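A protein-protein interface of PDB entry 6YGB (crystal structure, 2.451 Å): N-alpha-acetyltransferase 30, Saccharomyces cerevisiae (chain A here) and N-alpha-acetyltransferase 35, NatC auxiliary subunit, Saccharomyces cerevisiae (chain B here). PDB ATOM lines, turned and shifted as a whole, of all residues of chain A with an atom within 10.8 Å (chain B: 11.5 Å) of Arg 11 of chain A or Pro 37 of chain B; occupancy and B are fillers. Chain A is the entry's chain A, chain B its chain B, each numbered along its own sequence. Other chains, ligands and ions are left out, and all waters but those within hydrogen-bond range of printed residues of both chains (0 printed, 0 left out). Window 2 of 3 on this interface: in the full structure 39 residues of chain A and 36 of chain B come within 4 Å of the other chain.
Of the 12 printed residues of chain B, 4 touch a printed residue of chain A.
Printed residues of chain B that touch a printed residue of chain A: Pro 37, Glu 38, Ile 40 and Leu 48.
Of the 22 printed residues of chain A, 6 touch a printed residue of chain B.
Hydrophobic or aromatic side chains of chain A that line the printed part of chain B: Ile 10 and Tyr 38.
Among the printed residues, Asp or Glu carboxylates within 4 Å of a Lys or Arg side-chain nitrogen of the other chain: Arg 11 of chain A with Glu 38 of chain B (3.8 Å).
Among the printed residues, pairs that only touch across the chains: Asn 41 of chain A with Ile 40 of chain B, Tyr 38 of chain A with Leu 48 of chain B, Arg 11 of chain A with Pro 37 of chain B, Ile 10 of chain A with Glu 38 of chain B, Arg 37 of chain A with Pro 37 of chain B, Gln 42 of chain A with Leu 48 of chain B, Ile 10 of chain A with Pro 37 of chain B, Arg 37 of chain A with Ile 40 of chain B and Asn 41 of chain A with Pro 37 of chain B.
O of Glu 38 of chain B is in hydrogen-bond range of ND2 of Asn 41 of chain A (2.9 Å).
NH1 of Arg 11 of chain A lies within salt-bridge range of OE2 of Glu 38 of chain B, 3.8 Å away.
No residue of chain B comes within 4 Å of Asp 9 of chain A.
Arg 11 of chain A touches just these residues of chain B: Pro 37 and Glu 38.
Glu 13 of chain A touches none of the printed residues of chain B.
Of the printed residues of chain B, Arg 37 of chain A touches Pro 37 (3.7 Å) and Ile 40 (3.8 Å).
Printed residues of chain B within 4 Å of Gln 42 of chain A: Leu 48 (3.7 Å).
Pro 37 of chain B touches just these residues of chain A: Ile 10, Arg 11, Arg 37 and Asn 41.
Of the printed residues of chain A, Leu 48 of chain B touches Tyr 38 (3.5 Å) and Gln 42 (3.7 Å).
The nearest residue of chain B that does not touch Arg 11 of chain A is Lys 36 of chain B (5.0 Å).
The nearest residue of chain A that does not touch Pro 37 of chain B is Asn 12 of chain A (5.5 Å).
The nearest printed residue of chain B that does not touch Tyr 38 of chain A is Ile 40 of chain B (6.1 Å).
The guanidinium group (NH2) of Arg 37 of chain A is in salt-bridge range of the side-chain carboxylate (OE1) of Glu 13 of chain A.
OD1 of Asp 9 of chain A lies close to N of Arg 11 of chain A (3.4 Å).
The side-chain amide oxygen of Gln 42 of chain A lies close to the backbone carbonyl oxygen of Tyr 38 of chain A, at 3.2 Å.
The guanidinium group (NH1) of Arg 37 of chain A lies within hydrogen-bond range of the side-chain amide oxygen (OD1) of Asn 41 of chain A (2.9 Å).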
ATOM      1  N   PRO A   7      -0.618  -1.467 -18.871  1.00  0.00           N
ATOM      2  CA  PRO A   7       0.783  -1.226 -19.225  1.00  0.00           C
ATOM      3  C   PRO A   7       1.503  -0.429 -18.147  1.00  0.00           C
ATOM      4  O   PRO A   7       0.893   0.267 -17.332  1.00  0.00           O
ATOM      5  CB  PRO A   7       0.686  -0.416 -20.526  1.00  0.00           C
ATOM      6  CG  PRO A   7      -0.721  -0.618 -21.011  1.00  0.00           C
ATOM      7  CD  PRO A   7      -1.540  -0.768 -19.772  1.00  0.00           C
ATOM      8  N   LEU A   8       2.829  -0.546 -18.161  1.00  0.00           N
ATOM      9  CA  LEU A   8       3.665   0.159 -17.197  1.00  0.00           C
ATOM     10  C   LEU A   8       3.618   1.665 -17.420  1.00  0.00           C
ATOM     11  O   LEU A   8       3.658   2.141 -18.557  1.00  0.00           O
ATOM     12  CB  LEU A   8       5.111  -0.326 -17.300  1.00  0.00           C
ATOM     13  CG  LEU A   8       6.128   0.547 -16.564  1.00  0.00           C
ATOM     14  CD1 LEU A   8       6.161   0.208 -15.079  1.00  0.00           C
ATOM     15  CD2 LEU A   8       7.506   0.434 -17.192  1.00  0.00           C
ATOM     16  N   ASP A   9       3.536   2.414 -16.323  1.00  0.00           N
ATOM     17  CA  ASP A   9       3.672   3.866 -16.349  1.00  0.00           C
ATOM     18  C   ASP A   9       5.089   4.193 -15.902  1.00  0.00           C
ATOM     19  O   ASP A   9       5.424   4.021 -14.726  1.00  0.00           O
ATOM     20  CB  ASP A   9       2.653   4.542 -15.438  1.00  0.00           C
ATOM     21  CG  ASP A   9       2.632   6.044 -15.609  1.00  0.00           C
ATOM     22  OD1 ASP A   9       3.283   6.537 -16.555  1.00  0.00           O
ATOM     23  OD2 ASP A   9       1.965   6.730 -14.807  1.00  0.00           O
ATOM     24  N   ILE A  10       5.917   4.659 -16.840  1.00  0.00           N
ATOM     25  CA  ILE A  10       7.317   4.917 -16.525  1.00  0.00           C
ATOM     26  C   ILE A  10       7.452   6.083 -15.551  1.00  0.00           C
ATOM     27  O   ILE A  10       8.430   6.157 -14.793  1.00  0.00           O
ATOM     28  CB  ILE A  10       8.110   5.158 -17.826  1.00  0.00           C
ATOM     29  CG1 ILE A  10       9.616   5.103 -17.562  1.00  0.00           C
ATOM     30  CG2 ILE A  10       7.716   6.477 -18.476  1.00  0.00           C
ATOM     31  CD1 ILE A  10      10.109   3.739 -17.125  1.00  0.00           C
ATOM     32  N   ARG A  11       6.475   6.996 -15.533  1.00  0.00           N
ATOM     33  CA  ARG A  11       6.551   8.150 -14.645  1.00  0.00           C
ATOM     34  C   ARG A  11       6.262   7.782 -13.196  1.00  0.00           C
ATOM     35  O   ARG A  11       6.542   8.583 -12.299  1.00  0.00           O
ATOM     36  CB  ARG A  11       5.575   9.231 -15.103  1.00  0.00           C
ATOM     37  CG  ARG A  11       5.655   9.540 -16.588  1.00  0.00           C
ATOM     38  CD  ARG A  11       6.929  10.288 -16.943  1.00  0.00           C
ATOM     39  NE  ARG A  11       6.817  11.714 -16.653  1.00  0.00           N
ATOM     40  CZ  ARG A  11       6.586  12.648 -17.570  1.00  0.00           C
ATOM     41  NH1 ARG A  11       6.453  12.310 -18.847  1.00  0.00           N
ATOM     42  NH2 ARG A  11       6.495  13.922 -17.211  1.00  0.00           N
ATOM     43  N   ASN A  12       5.711   6.597 -12.947  1.00  0.00           N
ATOM     44  CA  ASN A  12       5.379   6.156 -11.595  1.00  0.00           C
ATOM     45  C   ASN A  12       6.601   5.454 -11.017  1.00  0.00           C
ATOM     46  O   ASN A  12       6.921   4.326 -11.392  1.00  0.00           O
ATOM     47  CB  ASN A  12       4.159   5.244 -11.621  1.00  0.00           C
ATOM     48  CG  ASN A  12       3.648   4.905 -10.232  1.00  0.00           C
ATOM     49  OD1 ASN A  12       4.381   4.986  -9.247  1.00  0.00           O
ATOM     50  ND2 ASN A  12       2.384   4.513 -10.152  1.00  0.00           N
ATOM     51  N   GLU A  13       7.291   6.133 -10.099  1.00  0.00           N
ATOM     52  CA  GLU A  13       8.432   5.523  -9.423  1.00  0.00           C
ATOM     53  C   GLU A  13       7.982   4.388  -8.514  1.00  0.00           C
ATOM     54  O   GLU A  13       8.661   3.361  -8.402  1.00  0.00           O
ATOM     55  CB  GLU A  13       9.196   6.585  -8.624  1.00  0.00           C
ATOM     56  CG  GLU A  13      10.298   6.036  -7.731  1.00  0.00           C
ATOM     57  CD  GLU A  13      11.505   5.550  -8.512  1.00  0.00           C
ATOM     58  OE1 GLU A  13      11.550   5.760  -9.742  1.00  0.00           O
ATOM     59  OE2 GLU A  13      12.415   4.961  -7.890  1.00  0.00           O
ATOM     60  N   GLU A  14       6.824   4.548  -7.873  1.00  0.00           N
ATOM     61  CA  GLU A  14       6.332   3.536  -6.945  1.00  0.00           C
ATOM     62  C   GLU A  14       5.954   2.252  -7.675  1.00  0.00           C
ATOM     63  O   GLU A  14       6.183   1.150  -7.165  1.00  0.00           O
ATOM     64  CB  GLU A  14       5.140   4.089  -6.168  1.00  0.00           C
ATOM     65  CG  GLU A  14       5.024   3.565  -4.753  1.00  0.00           C
ATOM     66  CD  GLU A  14       3.888   4.209  -3.990  1.00  0.00           C
ATOM     67  OE1 GLU A  14       2.957   4.733  -4.639  1.00  0.00           O
ATOM     68  OE2 GLU A  14       3.929   4.198  -2.742  1.00  0.00           O
ATOM     69  N   GLN A  15       5.362   2.380  -8.866  1.00  0.00           N
ATOM     70  CA  GLN A  15       5.080   1.212  -9.693  1.00  0.00           C
ATOM     71  C   GLN A  15       6.369   0.491 -10.068  1.00  0.00           C
ATOM     72  O   GLN A  15       6.438  -0.743 -10.020  1.00  0.00           O
ATOM     73  CB  GLN A  15       4.321   1.647 -10.947  1.00  0.00           C
ATOM     74  CG  GLN A  15       3.391   0.615 -11.554  1.00  0.00           C
ATOM     75  CD  GLN A  15       2.658   1.163 -12.766  1.00  0.00           C
ATOM     76  OE1 GLN A  15       3.271   1.473 -13.787  1.00  0.00           O
ATOM     77  NE2 GLN A  15       1.341   1.301 -12.652  1.00  0.00           N
ATOM     78  N   PHE A  16       7.400   1.255 -10.438  1.00  0.00           N
ATOM     79  CA  PHE A  16       8.702   0.679 -10.759  1.00  0.00           C
ATOM     80  C   PHE A  16       9.239  -0.151  -9.599  1.00  0.00           C
ATOM     81  O   PHE A  16       9.728  -1.270  -9.799  1.00  0.00           O
ATOM     82  CB  PHE A  16       9.676   1.806 -11.118  1.00  0.00           C
ATOM     83  CG  PHE A  16      11.009   1.333 -11.640  1.00  0.00           C
ATOM     84  CD1 PHE A  16      11.975   0.833 -10.781  1.00  0.00           C
ATOM     85  CD2 PHE A  16      11.309   1.432 -12.986  1.00  0.00           C
ATOM     86  CE1 PHE A  16      13.200   0.412 -11.261  1.00  0.00           C
ATOM     87  CE2 PHE A  16      12.536   1.014 -13.473  1.00  0.00           C
ATOM     88  CZ  PHE A  16      13.481   0.505 -12.608  1.00  0.00           C
ATOM     89  N   ALA A  17       9.157   0.381  -8.379  1.00  0.00           N
ATOM     90  CA  ALA A  17       9.742  -0.303  -7.229  1.00  0.00           C
ATOM     91  C   ALA A  17       8.951  -1.552  -6.861  1.00  0.00           C
ATOM     92  O   ALA A  17       9.536  -2.565  -6.460  1.00  0.00           O
ATOM     93  CB  ALA A  17       9.825   0.654  -6.039  1.00  0.00           C
ATOM     94  N   ILE A  19       7.382  -3.509  -8.914  1.00  0.00           N
ATOM     95  CA  ILE A  19       7.734  -4.547  -9.881  1.00  0.00           C
ATOM     96  C   ILE A  19       9.042  -5.215  -9.483  1.00  0.00           C
ATOM     97  O   ILE A  19       9.147  -6.446  -9.445  1.00  0.00           O
ATOM     98  CB  ILE A  19       7.827  -3.958 -11.298  1.00  0.00           C
ATOM     99  CG1 ILE A  19       6.449  -3.528 -11.797  1.00  0.00           C
ATOM    100  CG2 ILE A  19       8.472  -4.965 -12.243  1.00  0.00           C
ATOM    101  CD1 ILE A  19       6.501  -2.785 -13.109  1.00  0.00           C
ATOM    102  N   ILE A  33      19.310  -2.527 -10.177  1.00  0.00           N
ATOM    103  CA  ILE A  33      18.383  -1.518 -10.687  1.00  0.00           C
ATOM    104  C   ILE A  33      18.593  -1.303 -12.179  1.00  0.00           C
ATOM    105  O   ILE A  33      17.636  -1.115 -12.939  1.00  0.00           O
ATOM    106  CB  ILE A  33      18.537  -0.201  -9.903  1.00  0.00           C
ATOM    107  CG1 ILE A  33      17.943  -0.341  -8.499  1.00  0.00           C
ATOM    108  CG2 ILE A  33      17.898   0.962 -10.656  1.00  0.00           C
ATOM    109  CD1 ILE A  33      18.211   0.846  -7.598  1.00  0.00           C
ATOM    110  N   TYR A  34      19.846  -1.346 -12.625  1.00  0.00           N
ATOM    111  CA  TYR A  34      20.133  -1.074 -14.026  1.00  0.00           C
ATOM    112  C   TYR A  34      19.829  -2.255 -14.935  1.00  0.00           C
ATOM    113  O   TYR A  34      19.796  -2.085 -16.158  1.00  0.00           O
ATOM    114  CB  TYR A  34      21.583  -0.623 -14.189  1.00  0.00           C
ATOM    115  CG  TYR A  34      21.714   0.868 -14.042  1.00  0.00           C
ATOM    116  CD1 TYR A  34      21.923   1.446 -12.796  1.00  0.00           C
ATOM    117  CD2 TYR A  34      21.593   1.703 -15.143  1.00  0.00           C
ATOM    118  CE1 TYR A  34      22.028   2.812 -12.656  1.00  0.00           C
ATOM    119  CE2 TYR A  34      21.697   3.070 -15.012  1.00  0.00           C
ATOM    120  CZ  TYR A  34      21.914   3.619 -13.765  1.00  0.00           C
ATOM    121  OH  TYR A  34      22.017   4.980 -13.629  1.00  0.00           O
ATOM    122  N   TYR A  36      16.830  -3.584 -14.465  1.00  0.00           N
ATOM    123  CA  TYR A  36      15.455  -3.139 -14.660  1.00  0.00           C
ATOM    124  C   TYR A  36      15.398  -1.886 -15.528  1.00  0.00           C
ATOM    125  O   TYR A  36      14.476  -1.729 -16.336  1.00  0.00           O
ATOM    126  CB  TYR A  36      14.792  -2.891 -13.302  1.00  0.00           C
ATOM    127  CG  TYR A  36      14.540  -4.152 -12.498  1.00  0.00           C
ATOM    128  CD1 TYR A  36      13.436  -4.954 -12.758  1.00  0.00           C
ATOM    129  CD2 TYR A  36      15.400  -4.535 -11.474  1.00  0.00           C
ATOM    130  CE1 TYR A  36      13.197  -6.101 -12.028  1.00  0.00           C
ATOM    131  CE2 TYR A  36      15.168  -5.684 -10.740  1.00  0.00           C
ATOM    132  CZ  TYR A  36      14.065  -6.464 -11.023  1.00  0.00           C
ATOM    133  OH  TYR A  36      13.823  -7.610 -10.302  1.00  0.00           O
ATOM    134  N   ARG A  37      16.372  -0.982 -15.374  1.00  0.00           N
ATOM    135  CA  ARG A  37      16.402   0.228 -16.194  1.00  0.00           C
ATOM    136  C   ARG A  37      16.566  -0.110 -17.668  1.00  0.00           C
ATOM    137  O   ARG A  37      15.952   0.528 -18.531  1.00  0.00           O
ATOM    138  CB  ARG A  37      17.537   1.152 -15.743  1.00  0.00           C
ATOM    139  CG  ARG A  37      17.248   1.945 -14.480  1.00  0.00           C
ATOM    140  CD  ARG A  37      16.162   2.974 -14.720  1.00  0.00           C
ATOM    141  NE  ARG A  37      15.635   3.516 -13.472  1.00  0.00           N
ATOM    142  CZ  ARG A  37      14.560   4.292 -13.400  1.00  0.00           C
ATOM    143  NH1 ARG A  37      13.904   4.614 -14.506  1.00  0.00           N
ATOM    144  NH2 ARG A  37      14.140   4.746 -12.226  1.00  0.00           N
ATOM    145  N   TYR A  38      17.400  -1.108 -17.970  1.00  0.00           N
ATOM    146  CA  TYR A  38      17.645  -1.492 -19.358  1.00  0.00           C
ATOM    147  C   TYR A  38      16.356  -1.892 -20.064  1.00  0.00           C
ATOM    148  O   TYR A  38      16.131  -1.513 -21.219  1.00  0.00           O
ATOM    149  CB  TYR A  38      18.668  -2.628 -19.405  1.00  0.00           C
ATOM    150  CG  TYR A  38      18.658  -3.433 -20.687  1.00  0.00           C
ATOM    151  CD1 TYR A  38      19.249  -2.942 -21.844  1.00  0.00           C
ATOM    152  CD2 TYR A  38      18.071  -4.692 -20.735  1.00  0.00           C
ATOM    153  CE1 TYR A  38      19.246  -3.674 -23.013  1.00  0.00           C
ATOM    154  CE2 TYR A  38      18.064  -5.433 -21.899  1.00  0.00           C
ATOM    155  CZ  TYR A  38      18.652  -4.920 -23.037  1.00  0.00           C
ATOM    156  OH  TYR A  38      18.647  -5.657 -24.199  1.00  0.00           O
ATOM    157  N   LEU A  40      12.915  -1.373 -18.854  1.00  0.00           N
ATOM    158  CA  LEU A  40      11.741  -0.517 -18.709  1.00  0.00           C
ATOM    159  C   LEU A  40      11.928   0.855 -19.349  1.00  0.00           C
ATOM    160  O   LEU A  40      10.970   1.420 -19.889  1.00  0.00           O
ATOM    161  CB  LEU A  40      11.385  -0.368 -17.232  1.00  0.00           C
ATOM    162  CG  LEU A  40      10.506  -1.457 -16.607  1.00  0.00           C
ATOM    163  CD1 LEU A  40      11.166  -2.826 -16.669  1.00  0.00           C
ATOM    164  CD2 LEU A  40      10.173  -1.086 -15.170  1.00  0.00           C
ATOM    165  N   ASN A  41      13.136   1.419 -19.297  1.00  0.00           N
ATOM    166  CA  ASN A  41      13.323   2.743 -19.883  1.00  0.00           C
ATOM    167  C   ASN A  41      13.398   2.685 -21.401  1.00  0.00           C
ATOM    168  O   ASN A  41      12.943   3.613 -22.078  1.00  0.00           O
ATOM    169  CB  ASN A  41      14.571   3.417 -19.308  1.00  0.00           C
ATOM    170  CG  ASN A  41      14.365   3.898 -17.881  1.00  0.00           C
ATOM    171  OD1 ASN A  41      13.849   3.168 -17.036  1.00  0.00           O
ATOM    172  ND2 ASN A  41      14.759   5.141 -17.612  1.00  0.00           N
ATOM    173  N   GLN A  42      13.949   1.610 -21.954  1.00  0.00           N
ATOM    174  CA  GLN A  42      14.083   1.491 -23.397  1.00  0.00           C
ATOM    175  C   GLN A  42      12.868   0.861 -24.062  1.00  0.00           C
ATOM    176  O   GLN A  42      12.564   1.196 -25.214  1.00  0.00           O
ATOM    177  CB  GLN A  42      15.339   0.692 -23.747  1.00  0.00           C
ATOM    178  CG  GLN A  42      16.621   1.405 -23.365  1.00  0.00           C
ATOM    179  CD  GLN A  42      17.863   0.690 -23.854  1.00  0.00           C
ATOM    180  OE1 GLN A  42      18.052  -0.500 -23.600  1.00  0.00           O
ATOM    181  NE2 GLN A  42      18.721   1.417 -24.559  1.00  0.00           N
ATOM    182  N   PRO A  44       9.383   0.681 -22.564  1.00  0.00           N
ATOM    183  CA  PRO A  44       8.312   0.831 -21.563  1.00  0.00           C
ATOM    184  C   PRO A  44       6.999   0.193 -21.980  1.00  0.00           C
ATOM    185  O   PRO A  44       6.216  -0.223 -21.117  1.00  0.00           O
ATOM    186  CB  PRO A  44       8.186   2.354 -21.420  1.00  0.00           C
ATOM    187  CG  PRO A  44       8.682   2.886 -22.715  1.00  0.00           C
ATOM    188  CD  PRO A  44       9.794   1.979 -23.121  1.00  0.00           C
ATOM    189  N   GLU A  45       6.738   0.096 -23.282  1.00  0.00           N
ATOM    190  CA  GLU A  45       5.481  -0.447 -23.775  1.00  0.00           C
ATOM    191  C   GLU A  45       5.434  -1.971 -23.746  1.00  0.00           C
ATOM    192  O   GLU A  45       4.378  -2.545 -24.042  1.00  0.00           O
ATOM    193  CB  GLU A  45       5.221   0.049 -25.203  1.00  0.00           C
ATOM    194  CG  GLU A  45       6.147  -0.539 -26.272  1.00  0.00           C
ATOM    195  CD  GLU A  45       7.563   0.012 -26.216  1.00  0.00           C
ATOM    196  OE1 GLU A  45       7.822   0.938 -25.421  1.00  0.00           O
ATOM    197  OE2 GLU A  45       8.421  -0.487 -26.973  1.00  0.00           O
ATOM    198  N   LEU B  31      20.436  18.647 -10.573  1.00  0.00           N
ATOM    199  CA  LEU B  31      20.391  18.301 -11.989  1.00  0.00           C
ATOM    200  C   LEU B  31      19.482  17.103 -12.230  1.00  0.00           C
ATOM    201  O   LEU B  31      18.716  17.082 -13.201  1.00  0.00           O
ATOM    202  CB  LEU B  31      21.799  18.020 -12.515  1.00  0.00           C
ATOM    203  CG  LEU B  31      22.659  19.242 -12.842  1.00  0.00           C
ATOM    204  CD1 LEU B  31      23.985  18.814 -13.449  1.00  0.00           C
ATOM    205  CD2 LEU B  31      21.918  20.179 -13.783  1.00  0.00           C
ATOM    206  N   CYS B  32      19.541  16.101 -11.349  1.00  0.00           N
ATOM    207  CA  CYS B  32      18.677  14.932 -11.480  1.00  0.00           C
ATOM    208  C   CYS B  32      17.206  15.294 -11.325  1.00  0.00           C
ATOM    209  O   CYS B  32      16.343  14.644 -11.926  1.00  0.00           O
ATOM    210  CB  CYS B  32      19.075  13.866 -10.458  1.00  0.00           C
ATOM    211  SG  CYS B  32      20.566  12.938 -10.892  1.00  0.00           S
ATOM    212  N   SER B  33      16.899  16.319 -10.526  1.00  0.00           N
ATOM    213  CA  SER B  33      15.508  16.732 -10.360  1.00  0.00           C
ATOM    214  C   SER B  33      14.920  17.233 -11.671  1.00  0.00           C
ATOM    215  O   SER B  33      13.738  17.011 -11.956  1.00  0.00           O
ATOM    216  CB  SER B  33      15.395  17.815  -9.287  1.00  0.00           C
ATOM    217  OG  SER B  33      15.496  17.276  -7.981  1.00  0.00           O
ATOM    218  N   LYS B  34      15.730  17.920 -12.480  1.00  0.00           N
ATOM    219  CA  LYS B  34      15.242  18.434 -13.757  1.00  0.00           C
ATOM    220  C   LYS B  34      14.945  17.308 -14.733  1.00  0.00           C
ATOM    221  O   LYS B  34      14.107  17.466 -15.628  1.00  0.00           O
ATOM    222  CB  LYS B  34      16.262  19.403 -14.361  1.00  0.00           C
ATOM    223  CG  LYS B  34      16.580  20.605 -13.491  1.00  0.00           C
ATOM    224  CD  LYS B  34      17.717  21.426 -14.080  1.00  0.00           C
ATOM    225  CE  LYS B  34      18.057  22.612 -13.184  1.00  0.00           C
ATOM    226  NZ  LYS B  34      19.234  23.389 -13.671  1.00  0.00           N
ATOM    227  N   LEU B  35      15.611  16.172 -14.574  1.00  0.00           N
ATOM    228  CA  LEU B  35      15.443  15.060 -15.496  1.00  0.00           C
ATOM    229  C   LEU B  35      14.062  14.427 -15.361  1.00  0.00           C
ATOM    230  O   LEU B  35      13.472  14.372 -14.275  1.00  0.00           O
ATOM    231  CB  LEU B  35      16.512  13.998 -15.249  1.00  0.00           C
ATOM    232  CG  LEU B  35      17.946  14.358 -15.624  1.00  0.00           C
ATOM    233  CD1 LEU B  35      18.868  13.220 -15.227  1.00  0.00           C
ATOM    234  CD2 LEU B  35      18.057  14.656 -17.112  1.00  0.00           C
ATOM    235  N   LYS B  36      13.557  13.935 -16.489  1.00  0.00           N
ATOM    236  CA  LYS B  36      12.299  13.216 -16.558  1.00  0.00           C
ATOM    237  C   LYS B  36      12.478  11.794 -16.029  1.00  0.00           C
ATOM    238  O   LYS B  36      13.574  11.234 -16.105  1.00  0.00           O
ATOM    239  CB  LYS B  36      11.796  13.175 -17.997  1.00  0.00           C
ATOM    240  CG  LYS B  36      11.743  14.537 -18.665  1.00  0.00           C
ATOM    241  CD  LYS B  36      10.851  14.505 -19.895  1.00  0.00           C
ATOM    242  CE  LYS B  36      10.697  15.890 -20.501  1.00  0.00           C
ATOM    243  NZ  LYS B  36       9.642  15.922 -21.554  1.00  0.00           N
ATOM    244  N   PRO B  37      11.412  11.194 -15.484  1.00  0.00           N
ATOM    245  CA  PRO B  37      11.555   9.841 -14.915  1.00  0.00           C
ATOM    246  C   PRO B  37      12.107   8.828 -15.901  1.00  0.00           C
ATOM    247  O   PRO B  37      12.972   8.023 -15.535  1.00  0.00           O
ATOM    248  CB  PRO B  37      10.122   9.497 -14.482  1.00  0.00           C
ATOM    249  CG  PRO B  37       9.460  10.826 -14.276  1.00  0.00           C
ATOM    250  CD  PRO B  37      10.047  11.724 -15.323  1.00  0.00           C
ATOM    251  N   GLU B  38      11.643   8.860 -17.150  1.00  0.00           N
ATOM    252  CA  GLU B  38      12.096   7.912 -18.161  1.00  0.00           C
ATOM    253  C   GLU B  38      13.503   8.201 -18.661  1.00  0.00           C
ATOM    254  O   GLU B  38      14.092   7.347 -19.331  1.00  0.00           O
ATOM    255  CB  GLU B  38      11.127   7.909 -19.345  1.00  0.00           C
ATOM    256  CG  GLU B  38      11.135   9.197 -20.170  1.00  0.00           C
ATOM    257  CD  GLU B  38      10.235  10.286 -19.599  1.00  0.00           C
ATOM    258  OE1 GLU B  38      10.137  10.407 -18.359  1.00  0.00           O
ATOM    259  OE2 GLU B  38       9.617  11.023 -20.397  1.00  0.00           O
ATOM    260  N   ALA B  39      14.056   9.366 -18.348  1.00  0.00           N
ATOM    261  CA  ALA B  39      15.339   9.770 -18.898  1.00  0.00           C
ATOM    262  C   ALA B  39      16.505   9.049 -18.227  1.00  0.00           C
ATOM    263  O   ALA B  39      16.472   8.728 -17.037  1.00  0.00           O
ATOM    264  CB  ALA B  39      15.519  11.281 -18.756  1.00  0.00           C
ATOM    265  N   ILE B  40      17.549   8.803 -19.015  1.00  0.00           N
ATOM    266  CA  ILE B  40      18.802   8.240 -18.530  1.00  0.00           C
ATOM    267  C   ILE B  40      19.936   9.035 -19.151  1.00  0.00           C
ATOM    268  O   ILE B  40      19.999   9.174 -20.378  1.00  0.00           O
ATOM    269  CB  ILE B  40      18.954   6.750 -18.886  1.00  0.00           C
ATOM    270  CG1 ILE B  40      17.830   5.925 -18.259  1.00  0.00           C
ATOM    271  CG2 ILE B  40      20.327   6.244 -18.459  1.00  0.00           C
ATOM    272  CD1 ILE B  40      18.297   4.898 -17.246  1.00  0.00           C
ATOM    273  N   VAL B  41      20.827   9.552 -18.315  1.00  0.00           N
ATOM    274  CA  VAL B  41      22.001  10.265 -18.801  1.00  0.00           C
ATOM    275  C   VAL B  41      23.140   9.265 -18.896  1.00  0.00           C
ATOM    276  O   VAL B  41      23.463   8.589 -17.917  1.00  0.00           O
ATOM    277  CB  VAL B  41      22.364  11.440 -17.885  1.00  0.00           C
ATOM    278  CG1 VAL B  41      23.613  12.135 -18.392  1.00  0.00           C
ATOM    279  CG2 VAL B  41      21.213  12.420 -17.817  1.00  0.00           C
ATOM    280  N   LEU B  48      22.983   0.028 -22.769  1.00  0.00           N
ATOM    281  CA  LEU B  48      22.506  -0.284 -21.425  1.00  0.00           C
ATOM    282  C   LEU B  48      22.450  -1.780 -21.145  1.00  0.00           C
ATOM    283  O   LEU B  48      22.285  -2.171 -19.985  1.00  0.00           O
ATOM    284  CB  LEU B  48      21.130   0.346 -21.200  1.00  0.00           C
ATOM    285  CG  LEU B  48      21.157   1.854 -20.939  1.00  0.00           C
ATOM    286  CD1 LEU B  48      19.790   2.485 -21.171  1.00  0.00           C
ATOM    287  CD2 LEU B  48      21.643   2.130 -19.525  1.00  0.00           C
